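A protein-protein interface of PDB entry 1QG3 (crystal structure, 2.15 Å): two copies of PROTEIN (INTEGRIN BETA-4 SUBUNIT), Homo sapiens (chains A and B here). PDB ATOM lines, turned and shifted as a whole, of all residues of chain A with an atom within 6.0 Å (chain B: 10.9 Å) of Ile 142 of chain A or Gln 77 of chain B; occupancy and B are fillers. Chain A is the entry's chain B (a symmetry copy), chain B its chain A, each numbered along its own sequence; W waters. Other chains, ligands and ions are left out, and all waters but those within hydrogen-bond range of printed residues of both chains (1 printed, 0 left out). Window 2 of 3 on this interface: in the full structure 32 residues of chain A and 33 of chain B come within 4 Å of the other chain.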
ATOM      1  N   GLY A 133      -0.458  -6.634  21.255  1.00  0.00           N
ATOM      2  CA  GLY A 133      -0.683  -8.064  21.180  1.00  0.00           C
ATOM      3  C   GLY A 133      -1.269  -8.611  22.468  1.00  0.00           C
ATOM      4  O   GLY A 133      -1.290  -7.922  23.491  1.00  0.00           O
ATOM      5  N   LEU A 134      -1.738  -9.854  22.411  1.00  0.00           N
ATOM      6  CA  LEU A 134      -2.342 -10.530  23.554  1.00  0.00           C
ATOM      7  C   LEU A 134      -1.345 -10.826  24.666  1.00  0.00           C
ATOM      8  O   LEU A 134      -0.192 -11.148  24.396  1.00  0.00           O
ATOM      9  CB  LEU A 134      -2.967 -11.857  23.099  1.00  0.00           C
ATOM     10  CG  LEU A 134      -4.132 -11.810  22.106  1.00  0.00           C
ATOM     11  CD1 LEU A 134      -4.328 -13.183  21.486  1.00  0.00           C
ATOM     12  CD2 LEU A 134      -5.401 -11.354  22.816  1.00  0.00           C
ATOM     13  N   VAL A 135      -1.797 -10.721  25.914  1.00  0.00           N
ATOM     14  CA  VAL A 135      -0.958 -11.027  27.073  1.00  0.00           C
ATOM     15  C   VAL A 135      -1.713 -12.013  27.955  1.00  0.00           C
ATOM     16  O   VAL A 135      -2.936 -12.108  27.876  1.00  0.00           O
ATOM     17  CB  VAL A 135      -0.632  -9.773  27.936  1.00  0.00           C
ATOM     18  CG1 VAL A 135       0.204  -8.786  27.137  1.00  0.00           C
ATOM     19  CG2 VAL A 135      -1.917  -9.125  28.428  1.00  0.00           C
ATOM     20  N   ASN A 136      -0.984 -12.746  28.790  1.00  0.00           N
ATOM     21  CA  ASN A 136      -1.611 -13.709  29.689  1.00  0.00           C
ATOM     22  C   ASN A 136      -2.009 -13.025  30.989  1.00  0.00           C
ATOM     23  O   ASN A 136      -2.007 -11.800  31.082  1.00  0.00           O
ATOM     24  CB  ASN A 136      -0.660 -14.870  29.992  1.00  0.00           C
ATOM     25  CG  ASN A 136       0.690 -14.401  30.506  1.00  0.00           C
ATOM     26  OD1 ASN A 136       0.772 -13.497  31.335  1.00  0.00           O
ATOM     27  ND2 ASN A 136       1.756 -15.025  30.020  1.00  0.00           N
ATOM     28  N   ARG A 140       2.003 -10.956  30.419  1.00  0.00           N
ATOM     29  CA  ARG A 140       3.107 -11.425  29.591  1.00  0.00           C
ATOM     30  C   ARG A 140       2.613 -11.700  28.175  1.00  0.00           C
ATOM     31  O   ARG A 140       1.681 -12.477  27.974  1.00  0.00           O
ATOM     32  CB  ARG A 140       3.687 -12.719  30.171  1.00  0.00           C
ATOM     33  CG  ARG A 140       5.108 -12.614  30.692  1.00  0.00           C
ATOM     34  CD  ARG A 140       5.599 -13.954  31.231  1.00  0.00           C
ATOM     35  NE  ARG A 140       6.834 -14.395  30.585  1.00  0.00           N
ATOM     36  CZ  ARG A 140       7.535 -15.458  30.964  1.00  0.00           C
ATOM     37  NH1 ARG A 140       7.134 -16.193  31.990  1.00  0.00           N
ATOM     38  NH2 ARG A 140       8.636 -15.792  30.310  1.00  0.00           N
ATOM     39  N   PRO A 141       3.222 -11.055  27.174  1.00  0.00           N
ATOM     40  CA  PRO A 141       2.799 -11.281  25.792  1.00  0.00           C
ATOM     41  C   PRO A 141       2.716 -12.784  25.508  1.00  0.00           C
ATOM     42  O   PRO A 141       3.658 -13.531  25.794  1.00  0.00           O
ATOM     43  CB  PRO A 141       3.897 -10.596  24.990  1.00  0.00           C
ATOM     44  CG  PRO A 141       4.245  -9.424  25.866  1.00  0.00           C
ATOM     45  CD  PRO A 141       4.293 -10.043  27.245  1.00  0.00           C
ATOM     46  N   ILE A 142       1.586 -13.227  24.966  1.00  0.00           N
ATOM     47  CA  ILE A 142       1.393 -14.638  24.656  1.00  0.00           C
ATOM     48  C   ILE A 142       1.010 -14.828  23.195  1.00  0.00           C
ATOM     49  O   ILE A 142      -0.082 -15.308  22.883  1.00  0.00           O
ATOM     50  CB  ILE A 142       0.288 -15.268  25.538  1.00  0.00           C
ATOM     51  CG1 ILE A 142      -1.033 -14.519  25.339  1.00  0.00           C
ATOM     52  CG2 ILE A 142       0.707 -15.231  26.999  1.00  0.00           C
ATOM     53  CD1 ILE A 142      -2.237 -15.205  25.960  1.00  0.00           C
ATOM     54  N   GLY A 143       1.910 -14.451  22.295  1.00  0.00           N
ATOM     55  CA  GLY A 143       1.625 -14.594  20.880  1.00  0.00           C
ATOM     56  C   GLY A 143       2.373 -13.592  20.025  1.00  0.00           C
ATOM     57  O   GLY A 143       3.378 -13.027  20.461  1.00  0.00           O
ATOM     58  N   PRO A 144       1.912 -13.362  18.788  1.00  0.00           N
ATOM     59  CA  PRO A 144       2.566 -12.411  17.882  1.00  0.00           C
ATOM     60  C   PRO A 144       2.229 -10.952  18.203  1.00  0.00           C
ATOM     61  O   PRO A 144       1.166 -10.649  18.745  1.00  0.00           O
ATOM     62  CB  PRO A 144       2.042 -12.823  16.501  1.00  0.00           C
ATOM     63  CG  PRO A 144       1.618 -14.269  16.687  1.00  0.00           C
ATOM     64  CD  PRO A 144       0.979 -14.229  18.046  1.00  0.00           C
ATOM     65  N   ASP B   1       9.951 -22.246  26.105  1.00  0.00           N
ATOM     66  CA  ASP B   1      10.230 -21.250  25.038  1.00  0.00           C
ATOM     67  C   ASP B   1      11.619 -20.632  25.105  1.00  0.00           C
ATOM     68  O   ASP B   1      12.624 -21.330  25.254  1.00  0.00           O
ATOM     69  N   LEU B   2      11.676 -19.309  24.993  1.00  0.00           N
ATOM     70  CA  LEU B   2      12.944 -18.593  25.030  1.00  0.00           C
ATOM     71  C   LEU B   2      13.544 -18.546  26.428  1.00  0.00           C
ATOM     72  O   LEU B   2      12.838 -18.323  27.412  1.00  0.00           O
ATOM     73  CB  LEU B   2      12.755 -17.165  24.516  1.00  0.00           C
ATOM     74  CG  LEU B   2      12.466 -17.025  23.023  1.00  0.00           C
ATOM     75  CD1 LEU B   2      11.890 -15.654  22.733  1.00  0.00           C
ATOM     76  CD2 LEU B   2      13.747 -17.268  22.240  1.00  0.00           C
ATOM     77  N   GLY B   3      14.850 -18.765  26.507  1.00  0.00           N
ATOM     78  CA  GLY B   3      15.522 -18.710  27.790  1.00  0.00           C
ATOM     79  C   GLY B   3      15.795 -17.258  28.129  1.00  0.00           C
ATOM     80  O   GLY B   3      15.497 -16.361  27.328  1.00  0.00           O
ATOM     81  N   SER B  26      19.117 -19.225  24.347  1.00  0.00           N
ATOM     82  CA  SER B  26      18.914 -20.419  23.540  1.00  0.00           C
ATOM     83  C   SER B  26      17.604 -20.254  22.788  1.00  0.00           C
ATOM     84  O   SER B  26      16.638 -19.706  23.327  1.00  0.00           O
ATOM     85  CB  SER B  26      18.835 -21.650  24.444  1.00  0.00           C
ATOM     86  OG  SER B  26      17.915 -21.433  25.504  1.00  0.00           O
ATOM     87  N   GLY B  27      17.574 -20.714  21.541  1.00  0.00           N
ATOM     88  CA  GLY B  27      16.360 -20.599  20.755  1.00  0.00           C
ATOM     89  C   GLY B  27      16.455 -19.585  19.631  1.00  0.00           C
ATOM     90  O   GLY B  27      17.530 -19.363  19.071  1.00  0.00           O
ATOM     91  N   LYS B  28      15.324 -18.966  19.300  1.00  0.00           N
ATOM     92  CA  LYS B  28      15.284 -17.978  18.232  1.00  0.00           C
ATOM     93  C   LYS B  28      14.627 -16.673  18.656  1.00  0.00           C
ATOM     94  O   LYS B  28      13.442 -16.444  18.409  1.00  0.00           O
ATOM     95  CB  LYS B  28      14.550 -18.546  17.015  1.00  0.00           C
ATOM     96  CG  LYS B  28      15.348 -19.580  16.242  1.00  0.00           C
ATOM     97  CD  LYS B  28      14.587 -20.080  15.015  1.00  0.00           C
ATOM     98  CE  LYS B  28      14.238 -18.934  14.067  1.00  0.00           C
ATOM     99  NZ  LYS B  28      15.454 -18.185  13.625  1.00  0.00           N
ATOM    100  N   PRO B  29      15.396 -15.790  19.306  1.00  0.00           N
ATOM    101  CA  PRO B  29      14.851 -14.509  19.747  1.00  0.00           C
ATOM    102  C   PRO B  29      14.653 -13.616  18.530  1.00  0.00           C
ATOM    103  O   PRO B  29      15.444 -13.668  17.596  1.00  0.00           O
ATOM    104  CB  PRO B  29      15.947 -13.957  20.660  1.00  0.00           C
ATOM    105  CG  PRO B  29      16.784 -15.158  21.008  1.00  0.00           C
ATOM    106  CD  PRO B  29      16.793 -15.941  19.739  1.00  0.00           C
ATOM    107  N   MET B  30      13.597 -12.811  18.527  1.00  0.00           N
ATOM    108  CA  MET B  30      13.371 -11.899  17.415  1.00  0.00           C
ATOM    109  C   MET B  30      13.818 -10.501  17.832  1.00  0.00           C
ATOM    110  O   MET B  30      13.982  -9.620  16.996  1.00  0.00           O
ATOM    111  CB  MET B  30      11.892 -11.853  17.036  1.00  0.00           C
ATOM    112  CG  MET B  30      11.325 -13.156  16.525  1.00  0.00           C
ATOM    113  SD  MET B  30       9.652 -12.927  15.894  1.00  0.00           S
ATOM    114  CE  MET B  30       8.897 -12.009  17.254  1.00  0.00           C
ATOM    115  N   GLY B  31      14.000 -10.309  19.133  1.00  0.00           N
ATOM    116  CA  GLY B  31      14.424  -9.020  19.646  1.00  0.00           C
ATOM    117  C   GLY B  31      14.588  -9.080  21.149  1.00  0.00           C
ATOM    118  O   GLY B  31      14.574 -10.168  21.736  1.00  0.00           O
ATOM    119  N   ALA B  73      13.974 -11.629  26.286  1.00  0.00           N
ATOM    120  CA  ALA B  73      13.906 -11.832  24.840  1.00  0.00           C
ATOM    121  C   ALA B  73      12.465 -12.101  24.451  1.00  0.00           C
ATOM    122  O   ALA B  73      11.644 -12.438  25.299  1.00  0.00           O
ATOM    123  CB  ALA B  73      14.783 -13.014  24.433  1.00  0.00           C
ATOM    124  N   TYR B  74      12.150 -11.926  23.175  1.00  0.00           N
ATOM    125  CA  TYR B  74      10.808 -12.205  22.687  1.00  0.00           C
ATOM    126  C   TYR B  74      10.883 -12.806  21.288  1.00  0.00           C
ATOM    127  O   TYR B  74      11.853 -12.590  20.551  1.00  0.00           O
ATOM    128  CB  TYR B  74       9.930 -10.942  22.699  1.00  0.00           C
ATOM    129  CG  TYR B  74      10.397  -9.793  21.830  1.00  0.00           C
ATOM    130  CD1 TYR B  74      10.339  -9.872  20.440  1.00  0.00           C
ATOM    131  CD2 TYR B  74      10.869  -8.608  22.402  1.00  0.00           C
ATOM    132  CE1 TYR B  74      10.735  -8.803  19.633  1.00  0.00           C
ATOM    133  CE2 TYR B  74      11.274  -7.530  21.605  1.00  0.00           C
ATOM    134  CZ  TYR B  74      11.203  -7.635  20.220  1.00  0.00           C
ATOM    135  OH  TYR B  74      11.588  -6.577  19.422  1.00  0.00           O
ATOM    136  N   GLY B  75       9.861 -13.580  20.944  1.00  0.00           N
ATOM    137  CA  GLY B  75       9.810 -14.221  19.642  1.00  0.00           C
ATOM    138  C   GLY B  75       8.380 -14.502  19.210  1.00  0.00           C
ATOM    139  O   GLY B  75       7.467 -13.730  19.508  1.00  0.00           O
ATOM    140  N   ALA B  76       8.182 -15.621  18.520  1.00  0.00           N
ATOM    141  CA  ALA B  76       6.860 -15.998  18.029  1.00  0.00           C
ATOM    142  C   ALA B  76       5.846 -16.315  19.128  1.00  0.00           C
ATOM    143  O   ALA B  76       4.670 -15.970  19.012  1.00  0.00           O
ATOM    144  CB  ALA B  76       6.985 -17.187  17.087  1.00  0.00           C
ATOM    145  N   GLN B  77       6.303 -16.969  20.192  1.00  0.00           N
ATOM    146  CA  GLN B  77       5.431 -17.348  21.303  1.00  0.00           C
ATOM    147  C   GLN B  77       5.141 -16.204  22.274  1.00  0.00           C
ATOM    148  O   GLN B  77       4.069 -16.155  22.884  1.00  0.00           O
ATOM    149  CB  GLN B  77       6.043 -18.531  22.060  1.00  0.00           C
ATOM    150  CG  GLN B  77       6.023 -19.846  21.279  1.00  0.00           C
ATOM    151  CD  GLN B  77       6.603 -19.708  19.882  1.00  0.00           C
ATOM    152  OE1 GLN B  77       7.766 -19.340  19.710  1.00  0.00           O
ATOM    153  NE2 GLN B  77       5.789 -19.999  18.873  1.00  0.00           N
ATOM    154  N   GLY B  78       6.093 -15.287  22.410  1.00  0.00           N
ATOM    155  CA  GLY B  78       5.917 -14.158  23.309  1.00  0.00           C
ATOM    156  C   GLY B  78       7.227 -13.786  23.981  1.00  0.00           C
ATOM    157  O   GLY B  78       8.292 -13.937  23.380  1.00  0.00           O
ATOM    158  N   GLU B  79       7.154 -13.310  25.223  1.00  0.00           N
ATOM    159  CA  GLU B  79       8.356 -12.930  25.961  1.00  0.00           C
ATOM    160  C   GLU B  79       8.852 -14.035  26.881  1.00  0.00           C
ATOM    161  O   GLU B  79       8.063 -14.708  27.537  1.00  0.00           O
ATOM    162  CB  GLU B  79       8.111 -11.697  26.835  1.00  0.00           C
ATOM    163  CG  GLU B  79       7.736 -10.427  26.113  1.00  0.00           C
ATOM    164  CD  GLU B  79       7.854  -9.212  27.021  1.00  0.00           C
ATOM    165  OE1 GLU B  79       7.770  -9.377  28.255  1.00  0.00           O
ATOM    166  OE2 GLU B  79       8.024  -8.092  26.497  1.00  0.00           O
ATOM    167  N   GLY B  80      10.170 -14.203  26.929  1.00  0.00           N
ATOM    168  CA  GLY B  80      10.768 -15.185  27.811  1.00  0.00           C
ATOM    169  C   GLY B  80      11.063 -14.519  29.155  1.00  0.00           C
ATOM    170  O   GLY B  80      10.707 -13.358  29.365  1.00  0.00           O
ATOM    171  N   PRO B  81      11.730 -15.214  30.084  1.00  0.00           N
ATOM    172  CA  PRO B  81      12.037 -14.624  31.393  1.00  0.00           C
ATOM    173  C   PRO B  81      13.124 -13.553  31.352  1.00  0.00           C
ATOM    174  O   PRO B  81      13.970 -13.555  30.464  1.00  0.00           O
ATOM    175  CB  PRO B  81      12.449 -15.839  32.222  1.00  0.00           C
ATOM    176  CG  PRO B  81      13.140 -16.702  31.213  1.00  0.00           C
ATOM    177  CD  PRO B  81      12.249 -16.593  29.988  1.00  0.00           C
HETATM  178  O   HOH W   1       8.953 -11.821  31.035  1.00  0.00           O
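The guanidinium group (NH2) of Arg 140 of chain A sits close to the backbone carbonyl oxygen (O) of Gly 80 of chain B (3.3 Å). The backbone carbonyl oxygen of Gln 77 of chain B lies within hydrogen-bond range of the backbone NH of Gly 143 of chain A (2.8 Å). NH2 of Arg 140 of chain A sits at hydrogen-bond distance from O of Glu 79 of chain B, 3.0 Å away. The guanidinium group (NH2) of Arg 140 of chain A lies close to the backbone nitrogen (N) of Pro 81 of chain B.
N of Ile 142 of chain A lies within hydrogen-bond range of O of Leu 134 of chain A. N of Arg 140 of chain A sits at hydrogen-bond distance from OD1 of Asn 136 of chain A, 3.0 Å away. The backbone carbonyl oxygen (O) of Ala 73 of chain B sits at hydrogen-bond distance from the backbone NH (N) of Gly 80 of chain B, 2.8 Å away.
Among the printed residues, merely in contact across the chains: Ile 142 of chain A with Gln 77 of chain B, Pro 141 of chain A with Gly 78 of chain B, Gly 143 of chain A with Ala 76 of chain B, Pro 141 of chain A with Glu 79 of chain B, Pro 144 of chain A with Ala 76 of chain B, Pro 141 of chain A with Gln 77 of chain B and Gly 143 of chain A with Gly 78 of chain B.
Of chain B, only Gln 77 comes within 4 Å of Ile 142 of chain A. No residue of chain B comes within 4 Å of Asn 136 of chain A. Of chain B, only Gln 77, Gly 78 and Glu 79 come within 4 Å of Pro 141 of chain A. Printed residues of chain A within 4 Å of Gly 80 of chain B: Arg 140. Printed residues of chain A within 4 Å of Pro 81 of chain B: Arg 140. The nearest residue of chain A that does not touch Gln 77 of chain B is Pro 144 of chain A (5.4 Å). The nearest printed residue of chain A that does not touch Gly 80 of chain B is Pro 141 of chain A (6.6 Å).
Printed residues of chain A that touch a printed residue of chain B: Arg 140, Pro 141, Ile 142, Gly 143 and Pro 144. Hydrophobic or aromatic side chains of chain A within 4 Å of the printed part of chain B: Pro 141.
No position is printed for both chains. Of the 11 pairs that touch across the chains among the printed residues, none has its exchanged pair printed and touching as well.
Water W1 lies within hydrogen-bond range of O of Gly 80 of chain B (2.9 Å) and NE of Arg 140 of chain A (3.4 Å).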
